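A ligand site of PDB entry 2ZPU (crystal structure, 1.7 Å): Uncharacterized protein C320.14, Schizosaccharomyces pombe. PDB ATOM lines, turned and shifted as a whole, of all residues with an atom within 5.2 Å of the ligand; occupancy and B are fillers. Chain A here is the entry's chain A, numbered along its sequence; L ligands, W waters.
The side-chain amino group (NZ) of Lys 57 is covalently linked to a carbon (C10) of the ligand (1.4 Å). OG of Ser 81 lies within hydrogen-bond range of O7 of the ligand (2.5 Å). A nitrogen (N2) of the ligand sits at hydrogen-bond distance from the side-chain hydroxyl (OG) of Ser 308. O5 of the ligand sits at hydrogen-bond distance from N of Gly 185 (2.6 Å). The backbone NH (N) of Asn 84 is in hydrogen-bond range of an oxygen (O6) of the ligand, 3.1 Å away. ND2 of Asn 84 lies within hydrogen-bond range of O1 of the ligand, 2.7 Å away. The backbone NH (N) of Gly 184 sits at hydrogen-bond distance from an oxygen (O3) of the ligand (2.8 Å). The backbone NH (N) of Gly 183 lies within hydrogen-bond range of an oxygen (O5) of the ligand, at 2.9 Å. An oxygen (O6) of the ligand lies within hydrogen-bond range of the backbone NH (N) of His 85 (2.9 Å). The backbone NH of Gly 186 is in hydrogen-bond range of an oxygen (O4) of the ligand, at 3.0 Å. An oxygen (O4) of the ligand lies within hydrogen-bond range of the backbone NH (N) of Leu 187, 3.1 Å away. N of Ser 82 sits at hydrogen-bond distance from O7 of the ligand, 3.2 Å away. The side-chain hydroxyl (OG) of Ser 82 is in hydrogen-bond range of an oxygen (O6) of the ligand (3.1 Å).
The side-chain amino group (NZ) of Lys 57 lies within hydrogen-bond range of the backbone carbonyl oxygen (O) of Pro 151 (2.8 Å). The side-chain hydroxyl (OG) of Ser 81 sits at hydrogen-bond distance from the backbone NH (N) of Gly 83 (2.9 Å). The backbone carbonyl oxygen (O) of Ser 308 sits at hydrogen-bond distance from the backbone NH (N) of Phe 56 (3.0 Å). ND2 of Asn 84 is in hydrogen-bond range of OE2 of Glu 281 (3.0 Å). OG1 of Thr 283 lies within hydrogen-bond range of N of Gly 236, 2.9 Å away. O of Gly 309 sits at hydrogen-bond distance from N of Glu 281 (3.1 Å). NZ of Lys 112 lies within salt-bridge range of OE1 of Glu 281 (2.9 Å). The side-chain hydroxyl of Tyr 152 sits at hydrogen-bond distance from the guanidinium group of Arg 133 (3.4 Å).
Residues that only touch the ligand: Phe 56 (3.6 Å), Gly 83 (3.7 Å), Pro 151 (3.3 Å), Tyr 152 (3.8 Å), Cys 181 (3.6 Å), Leu 182 (3.98 Å), Gly 236 (3.1 Å), Glu 281 (3.4 Å), Thr 283 (3.4 Å) and Gly 309 (3.8 Å). Hydrophobic or aromatic side chains within 4 Å of the ligand: Phe 56, His 85, Pro 151 and Tyr 152. Within 4 Å of the ligand: Phe 56, Lys 57, Ser 81, Ser 82, Gly 83, Asn 84, His 85, Pro 151, Tyr 152, Cys 181, Leu 182, Gly 183, Gly 184, Gly 185, Gly 186, Leu 187, Gly 236, Glu 281, Thr 283, Ser 308 and Gly 309.
Water W3 lies within hydrogen-bond range of an oxygen (O3) of the ligand (2.7 Å), the backbone carbonyl oxygen of Gly 236 (2.8 Å) and the backbone NH of Gly 184 (3.5 Å). Water W4 lies within hydrogen-bond range of N of Leu 188 (2.7 Å), O5 of the ligand (2.8 Å) and O of Cys 181 (2.8 Å). Water W2 lies within hydrogen-bond range of the backbone carbonyl oxygen of Pro 151 (2.7 Å), an oxygen (O4) of the ligand (2.8 Å) and the side-chain amino group of Lys 57 (3.3 Å). Water W1 lies within hydrogen-bond range of the side-chain amino group (NZ) of Lys 112, an oxygen (O1) of the ligand, the side-chain hydroxyl (OG) of Ser 82 and the backbone NH (N) of Asn 84. Water W5 lies within hydrogen-bond range of NH1 of Arg 133 (2.9 Å), O7 of the ligand (2.9 Å) and N of Ser 82 (3.4 Å).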
ATOM      1  N   ALA A  55     -18.467  -3.524  11.370  1.00  0.00           N
ATOM      2  CA  ALA A  55     -17.808  -2.218  11.451  1.00  0.00           C
ATOM      3  C   ALA A  55     -17.463  -1.870  12.892  1.00  0.00           C
ATOM      4  O   ALA A  55     -17.994  -2.463  13.829  1.00  0.00           O
ATOM      5  CB  ALA A  55     -18.698  -1.131  10.833  1.00  0.00           C
ATOM      6  N   PHE A  56     -16.572  -0.902  13.057  1.00  0.00           N
ATOM      7  CA  PHE A  56     -16.138  -0.475  14.380  1.00  0.00           C
ATOM      8  C   PHE A  56     -17.259   0.072  15.252  1.00  0.00           C
ATOM      9  O   PHE A  56     -17.171   0.059  16.477  1.00  0.00           O
ATOM     10  CB  PHE A  56     -15.049   0.600  14.236  1.00  0.00           C
ATOM     11  CG  PHE A  56     -15.581   1.931  13.797  1.00  0.00           C
ATOM     12  CD1 PHE A  56     -15.962   2.897  14.734  1.00  0.00           C
ATOM     13  CD2 PHE A  56     -15.702   2.241  12.442  1.00  0.00           C
ATOM     14  CE1 PHE A  56     -16.445   4.137  14.334  1.00  0.00           C
ATOM     15  CE2 PHE A  56     -16.181   3.472  12.027  1.00  0.00           C
ATOM     16  CZ  PHE A  56     -16.554   4.435  12.981  1.00  0.00           C
ATOM     17  N   LYS A  57     -18.320   0.549  14.611  1.00  0.00           N
ATOM     18  CA  LYS A  57     -19.456   1.164  15.312  1.00  0.00           C
ATOM     19  C   LYS A  57     -20.066   0.423  16.483  1.00  0.00           C
ATOM     20  O   LYS A  57     -20.655   1.039  17.374  1.00  0.00           O
ATOM     21  CB  LYS A  57     -20.563   1.485  14.304  1.00  0.00           C
ATOM     22  CG  LYS A  57     -20.217   2.589  13.326  1.00  0.00           C
ATOM     23  CD  LYS A  57     -20.191   3.963  13.979  1.00  0.00           C
ATOM     24  CE  LYS A  57     -20.095   5.024  12.899  1.00  0.00           C
ATOM     25  NZ  LYS A  57     -20.531   6.416  13.168  1.00  0.00           N
ATOM     26  N   PHE A  80     -29.690   8.486  14.225  1.00  0.00           N
ATOM     27  CA  PHE A  80     -29.662   8.790  12.810  1.00  0.00           C
ATOM     28  C   PHE A  80     -28.292   8.310  12.360  1.00  0.00           C
ATOM     29  O   PHE A  80     -27.288   8.555  13.030  1.00  0.00           O
ATOM     30  CB  PHE A  80     -29.862  10.288  12.548  1.00  0.00           C
ATOM     31  CG  PHE A  80     -29.057  11.199  13.439  1.00  0.00           C
ATOM     32  CD1 PHE A  80     -27.826  11.702  13.018  1.00  0.00           C
ATOM     33  CD2 PHE A  80     -29.547  11.572  14.686  1.00  0.00           C
ATOM     34  CE1 PHE A  80     -27.096  12.572  13.824  1.00  0.00           C
ATOM     35  CE2 PHE A  80     -28.813  12.440  15.502  1.00  0.00           C
ATOM     36  CZ  PHE A  80     -27.588  12.936  15.070  1.00  0.00           C
ATOM     37  N   SER A  81     -28.248   7.606  11.240  1.00  0.00           N
ATOM     38  CA  SER A  81     -26.995   7.036  10.784  1.00  0.00           C
ATOM     39  C   SER A  81     -26.968   6.668   9.309  1.00  0.00           C
ATOM     40  O   SER A  81     -27.997   6.311   8.730  1.00  0.00           O
ATOM     41  CB  SER A  81     -26.706   5.793  11.613  1.00  0.00           C
ATOM     42  OG  SER A  81     -25.750   4.951  10.988  1.00  0.00           O
ATOM     43  N   SER A  82     -25.786   6.734   8.715  1.00  0.00           N
ATOM     44  CA  SER A  82     -25.615   6.384   7.310  1.00  0.00           C
ATOM     45  C   SER A  82     -25.771   4.872   7.131  1.00  0.00           C
ATOM     46  O   SER A  82     -25.918   4.377   6.017  1.00  0.00           O
ATOM     47  CB  SER A  82     -24.237   6.824   6.806  1.00  0.00           C
ATOM     48  OG  SER A  82     -23.213   6.407   7.690  1.00  0.00           O
ATOM     49  N   GLY A  83     -25.743   4.129   8.246  1.00  0.00           N
ATOM     50  CA  GLY A  83     -25.924   2.702   8.128  1.00  0.00           C
ATOM     51  C   GLY A  83     -25.213   1.801   9.125  1.00  0.00           C
ATOM     52  O   GLY A  83     -25.800   0.841   9.615  1.00  0.00           O
ATOM     53  N   ASN A  84     -23.953   2.095   9.425  1.00  0.00           N
ATOM     54  CA  ASN A  84     -23.236   1.252  10.362  1.00  0.00           C
ATOM     55  C   ASN A  84     -23.596   1.512  11.818  1.00  0.00           C
ATOM     56  O   ASN A  84     -23.763   0.565  12.583  1.00  0.00           O
ATOM     57  CB  ASN A  84     -21.726   1.361  10.104  1.00  0.00           C
ATOM     58  CG  ASN A  84     -21.313   0.600   8.854  1.00  0.00           C
ATOM     59  OD1 ASN A  84     -21.886  -0.448   8.545  1.00  0.00           O
ATOM     60  ND2 ASN A  84     -20.303   1.106   8.133  1.00  0.00           N
ATOM     61  N   HIS A  85     -23.709   2.775  12.212  1.00  0.00           N
ATOM     62  CA  HIS A  85     -24.095   3.079  13.587  1.00  0.00           C
ATOM     63  C   HIS A  85     -25.527   2.551  13.752  1.00  0.00           C
ATOM     64  O   HIS A  85     -25.920   2.097  14.829  1.00  0.00           O
ATOM     65  CB  HIS A  85     -24.056   4.594  13.822  1.00  0.00           C
ATOM     66  CG  HIS A  85     -24.394   4.991  15.226  1.00  0.00           C
ATOM     67  ND1 HIS A  85     -23.622   4.638  16.320  1.00  0.00           N
ATOM     68  CD2 HIS A  85     -25.404   5.756  15.716  1.00  0.00           C
ATOM     69  CE1 HIS A  85     -24.141   5.168  17.408  1.00  0.00           C
ATOM     70  NE2 HIS A  85     -25.227   5.847  17.075  1.00  0.00           N
ATOM     71  N   ALA A  86     -26.300   2.608  12.669  1.00  0.00           N
ATOM     72  CA  ALA A  86     -27.677   2.118  12.669  1.00  0.00           C
ATOM     73  C   ALA A  86     -27.714   0.652  13.083  1.00  0.00           C
ATOM     74  O   ALA A  86     -28.436   0.271  14.004  1.00  0.00           O
ATOM     75  CB  ALA A  86     -28.296   2.287  11.276  1.00  0.00           C
ATOM     76  N   LYS A 112     -27.056  -2.584   4.722  1.00  0.00           N
ATOM     77  CA  LYS A 112     -27.046  -1.898   6.004  1.00  0.00           C
ATOM     78  C   LYS A 112     -28.468  -1.676   6.519  1.00  0.00           C
ATOM     79  O   LYS A 112     -28.730  -1.774   7.714  1.00  0.00           O
ATOM     80  CB  LYS A 112     -26.318  -0.551   5.902  1.00  0.00           C
ATOM     81  CG  LYS A 112     -24.825  -0.675   5.574  1.00  0.00           C
ATOM     82  CD  LYS A 112     -24.135   0.673   5.625  1.00  0.00           C
ATOM     83  CE  LYS A 112     -22.659   0.560   5.240  1.00  0.00           C
ATOM     84  NZ  LYS A 112     -21.988   1.885   5.251  1.00  0.00           N
ATOM     85  N   ARG A 133     -31.393  15.664   8.937  1.00  0.00           N
ATOM     86  CA  ARG A 133     -31.676  14.497   9.749  1.00  0.00           C
ATOM     87  C   ARG A 133     -31.669  14.756  11.254  1.00  0.00           C
ATOM     88  O   ARG A 133     -32.354  14.071  12.012  1.00  0.00           O
ATOM     89  CB  ARG A 133     -30.684  13.375   9.424  1.00  0.00           C
ATOM     90  CG  ARG A 133     -29.250  13.709   9.761  1.00  0.00           C
ATOM     91  CD  ARG A 133     -28.338  12.575   9.361  1.00  0.00           C
ATOM     92  NE  ARG A 133     -26.983  12.760   9.864  1.00  0.00           N
ATOM     93  CZ  ARG A 133     -26.084  11.791   9.939  1.00  0.00           C
ATOM     94  NH1 ARG A 133     -26.394  10.569   9.540  1.00  0.00           N
ATOM     95  NH2 ARG A 133     -24.880  12.041  10.447  1.00  0.00           N
ATOM     96  N   PRO A 151     -24.486   9.290  16.152  1.00  0.00           N
ATOM     97  CA  PRO A 151     -23.528   8.426  15.466  1.00  0.00           C
ATOM     98  C   PRO A 151     -22.052   8.760  15.704  1.00  0.00           C
ATOM     99  O   PRO A 151     -21.185   7.934  15.450  1.00  0.00           O
ATOM    100  CB  PRO A 151     -23.948   8.555  14.005  1.00  0.00           C
ATOM    101  CG  PRO A 151     -24.487   9.948  13.919  1.00  0.00           C
ATOM    102  CD  PRO A 151     -25.316  10.035  15.193  1.00  0.00           C
ATOM    103  N   TYR A 152     -21.780   9.970  16.209  1.00  0.00           N
ATOM    104  CA  TYR A 152     -20.400  10.336  16.499  1.00  0.00           C
ATOM    105  C   TYR A 152     -20.205  11.459  17.518  1.00  0.00           C
ATOM    106  O   TYR A 152     -19.296  11.388  18.331  1.00  0.00           O
ATOM    107  CB  TYR A 152     -19.632  10.693  15.214  1.00  0.00           C
ATOM    108  CG  TYR A 152     -20.364  11.610  14.264  1.00  0.00           C
ATOM    109  CD1 TYR A 152     -20.382  12.995  14.456  1.00  0.00           C
ATOM    110  CD2 TYR A 152     -21.075  11.094  13.178  1.00  0.00           C
ATOM    111  CE1 TYR A 152     -21.091  13.838  13.582  1.00  0.00           C
ATOM    112  CE2 TYR A 152     -21.782  11.915  12.311  1.00  0.00           C
ATOM    113  CZ  TYR A 152     -21.779  13.275  12.522  1.00  0.00           C
ATOM    114  OH  TYR A 152     -22.497  14.076  11.656  1.00  0.00           O
ATOM    115  N   CYS A 181     -10.083   6.707   9.194  1.00  0.00           N
ATOM    116  CA  CYS A 181     -11.140   7.189   8.305  1.00  0.00           C
ATOM    117  C   CYS A 181     -11.903   8.315   9.015  1.00  0.00           C
ATOM    118  O   CYS A 181     -12.079   8.268  10.224  1.00  0.00           O
ATOM    119  CB  CYS A 181     -12.097   6.026   7.989  1.00  0.00           C
ATOM    120  SG  CYS A 181     -11.273   4.457   7.569  1.00  0.00           S
ATOM    121  N   LEU A 182     -12.350   9.329   8.263  1.00  0.00           N
ATOM    122  CA  LEU A 182     -13.044  10.461   8.885  1.00  0.00           C
ATOM    123  C   LEU A 182     -14.373  10.910   8.265  1.00  0.00           C
ATOM    124  O   LEU A 182     -14.419  11.315   7.106  1.00  0.00           O
ATOM    125  CB  LEU A 182     -12.118  11.684   8.947  1.00  0.00           C
ATOM    126  CG  LEU A 182     -12.722  12.998   9.449  1.00  0.00           C
ATOM    127  CD1 LEU A 182     -13.226  12.828  10.881  1.00  0.00           C
ATOM    128  CD2 LEU A 182     -11.676  14.104   9.398  1.00  0.00           C
ATOM    129  N   GLY A 183     -15.424  10.822   9.062  1.00  0.00           N
ATOM    130  CA  GLY A 183     -16.747  11.268   8.663  1.00  0.00           C
ATOM    131  C   GLY A 183     -17.055  12.393   9.651  1.00  0.00           C
ATOM    132  O   GLY A 183     -16.573  13.507   9.488  1.00  0.00           O
ATOM    133  N   GLY A 184     -17.834  12.074  10.680  1.00  0.00           N
ATOM    134  CA  GLY A 184     -18.174  13.054  11.701  1.00  0.00           C
ATOM    135  C   GLY A 184     -17.084  13.257  12.738  1.00  0.00           C
ATOM    136  O   GLY A 184     -17.101  14.247  13.484  1.00  0.00           O
ATOM    137  N   GLY A 185     -16.123  12.326  12.801  1.00  0.00           N
ATOM    138  CA  GLY A 185     -15.024  12.461  13.743  1.00  0.00           C
ATOM    139  C   GLY A 185     -15.021  11.572  14.976  1.00  0.00           C
ATOM    140  O   GLY A 185     -14.124  11.700  15.822  1.00  0.00           O
ATOM    141  N   GLY A 186     -16.019  10.692  15.115  1.00  0.00           N
ATOM    142  CA  GLY A 186     -16.075   9.820  16.268  1.00  0.00           C
ATOM    143  C   GLY A 186     -14.912   8.841  16.316  1.00  0.00           C
ATOM    144  O   GLY A 186     -14.230   8.721  17.329  1.00  0.00           O
ATOM    145  N   LEU A 187     -14.682   8.147  15.211  1.00  0.00           N
ATOM    146  CA  LEU A 187     -13.593   7.180  15.151  1.00  0.00           C
ATOM    147  C   LEU A 187     -12.243   7.881  15.316  1.00  0.00           C
ATOM    148  O   LEU A 187     -11.393   7.418  16.072  1.00  0.00           O
ATOM    149  CB  LEU A 187     -13.633   6.411  13.834  1.00  0.00           C
ATOM    150  CG  LEU A 187     -12.485   5.427  13.573  1.00  0.00           C
ATOM    151  CD1 LEU A 187     -12.521   4.287  14.599  1.00  0.00           C
ATOM    152  CD2 LEU A 187     -12.610   4.882  12.160  1.00  0.00           C
ATOM    153  N   LEU A 188     -12.068   9.010  14.627  1.00  0.00           N
ATOM    154  CA  LEU A 188     -10.817   9.744  14.700  1.00  0.00           C
ATOM    155  C   LEU A 188     -10.547  10.330  16.087  1.00  0.00           C
ATOM    156  O   LEU A 188      -9.442  10.210  16.618  1.00  0.00           O
ATOM    157  CB  LEU A 188     -10.791  10.867  13.654  1.00  0.00           C
ATOM    158  CG  LEU A 188      -9.509  11.725  13.624  1.00  0.00           C
ATOM    159  CD1 LEU A 188      -8.300  10.854  13.390  1.00  0.00           C
ATOM    160  CD2 LEU A 188      -9.629  12.777  12.532  1.00  0.00           C
ATOM    161  N   GLY A 236     -20.057   6.254   4.241  1.00  0.00           N
ATOM    162  CA  GLY A 236     -20.014   6.447   5.684  1.00  0.00           C
ATOM    163  C   GLY A 236     -19.241   7.714   6.029  1.00  0.00           C
ATOM    164  O   GLY A 236     -18.920   7.962   7.193  1.00  0.00           O
ATOM    165  N   GLU A 281     -15.428  -1.970   2.798  1.00  0.00           N
ATOM    166  CA  GLU A 281     -16.301  -1.037   2.109  1.00  0.00           C
ATOM    167  C   GLU A 281     -15.482   0.197   1.741  1.00  0.00           C
ATOM    168  O   GLU A 281     -14.452   0.469   2.348  1.00  0.00           O
ATOM    169  CB  GLU A 281     -17.521  -0.672   2.971  1.00  0.00           C
ATOM    170  CG  GLU A 281     -17.242  -0.128   4.357  1.00  0.00           C
ATOM    171  CD  GLU A 281     -18.519   0.189   5.102  1.00  0.00           C
ATOM    172  OE1 GLU A 281     -19.191   1.189   4.735  1.00  0.00           O
ATOM    173  OE2 GLU A 281     -18.856  -0.546   6.055  1.00  0.00           O
ATOM    174  N   THR A 283     -15.621   3.369   2.352  1.00  0.00           N
ATOM    175  CA  THR A 283     -15.242   4.261   3.442  1.00  0.00           C
ATOM    176  C   THR A 283     -14.099   3.687   4.284  1.00  0.00           C
ATOM    177  O   THR A 283     -13.255   4.436   4.800  1.00  0.00           O
ATOM    178  CB  THR A 283     -16.454   4.570   4.345  1.00  0.00           C
ATOM    179  OG1 THR A 283     -17.562   5.004   3.539  1.00  0.00           O
ATOM    180  CG2 THR A 283     -16.121   5.684   5.330  1.00  0.00           C
ATOM    181  N   GLY A 284     -14.051   2.366   4.404  1.00  0.00           N
ATOM    182  CA  GLY A 284     -13.003   1.727   5.189  1.00  0.00           C
ATOM    183  C   GLY A 284     -11.669   1.684   4.480  1.00  0.00           C
ATOM    184  O   GLY A 284     -10.674   1.206   5.029  1.00  0.00           O
ATOM    185  N   SER A 308     -11.972   0.336   9.007  1.00  0.00           N
ATOM    186  CA  SER A 308     -13.221   0.659   9.695  1.00  0.00           C
ATOM    187  C   SER A 308     -14.441  -0.234   9.510  1.00  0.00           C
ATOM    188  O   SER A 308     -15.228  -0.407  10.446  1.00  0.00           O
ATOM    189  CB  SER A 308     -13.617   2.103   9.371  1.00  0.00           C
ATOM    190  OG  SER A 308     -13.869   2.267   7.982  1.00  0.00           O
ATOM    191  N   GLY A 309     -14.625  -0.796   8.322  1.00  0.00           N
ATOM    192  CA  GLY A 309     -15.782  -1.650   8.104  1.00  0.00           C
ATOM    193  C   GLY A 309     -15.781  -2.361   6.778  1.00  0.00           C
ATOM    194  O   GLY A 309     -14.979  -2.065   5.891  1.00  0.00           O
HETATM  195  N1  LIG L   1     -20.291   5.985  10.243  1.00  0.00           N
HETATM  196  N2  LIG L   1     -15.770   3.980   8.255  1.00  0.00           N
HETATM  197  C1  LIG L   1     -17.017   3.329   8.163  1.00  0.00           C
HETATM  198  C2  LIG L   1     -17.114   1.973   7.569  1.00  0.00           C
HETATM  199  C3  LIG L   1     -18.220   4.059   8.670  1.00  0.00           C
HETATM  200  O1  LIG L   1     -19.491   3.602   8.659  1.00  0.00           O
HETATM  201  C4  LIG L   1     -17.981   5.453   9.259  1.00  0.00           C
HETATM  202  C5  LIG L   1     -19.106   6.292   9.806  1.00  0.00           C
HETATM  203  C6  LIG L   1     -16.647   6.021   9.305  1.00  0.00           C
HETATM  204  C7  LIG L   1     -16.390   7.405   9.884  1.00  0.00           C
HETATM  205  O2  LIG L   1     -16.670   7.605  11.279  1.00  0.00           O
HETATM  206  P1  LIG L   1     -16.858   8.864  11.887  1.00  0.00           P
HETATM  207  O3  LIG L   1     -18.160   9.356  11.297  1.00  0.00           O
HETATM  208  O4  LIG L   1     -17.060   8.603  13.259  1.00  0.00           O
HETATM  209  O5  LIG L   1     -16.027   9.971  11.759  1.00  0.00           O
HETATM  210  C8  LIG L   1     -15.524   5.248   8.794  1.00  0.00           C
HETATM  211  C9  LIG L   1     -21.375   6.831  10.783  1.00  0.00           C
HETATM  212  C10 LIG L   1     -21.118   7.251  12.201  1.00  0.00           C
HETATM  213  C11 LIG L   1     -22.748   6.016  10.786  1.00  0.00           C
HETATM  214  O6  LIG L   1     -22.788   4.849  10.393  1.00  0.00           O
HETATM  215  O7  LIG L   1     -23.809   6.525  11.185  1.00  0.00           O
HETATM  216  O   HOH W   1     -22.069   3.727   7.369  1.00  0.00           O
HETATM  217  O   HOH W   2     -18.490   7.596  15.466  1.00  0.00           O
HETATM  218  O   HOH W   3     -19.812   9.642   9.203  1.00  0.00           O
HETATM  219  O   HOH W   4     -13.346   9.647  12.323  1.00  0.00           O
HETATM  220  O   HOH W   5     -23.947   9.224  10.156  1.00  0.00           O
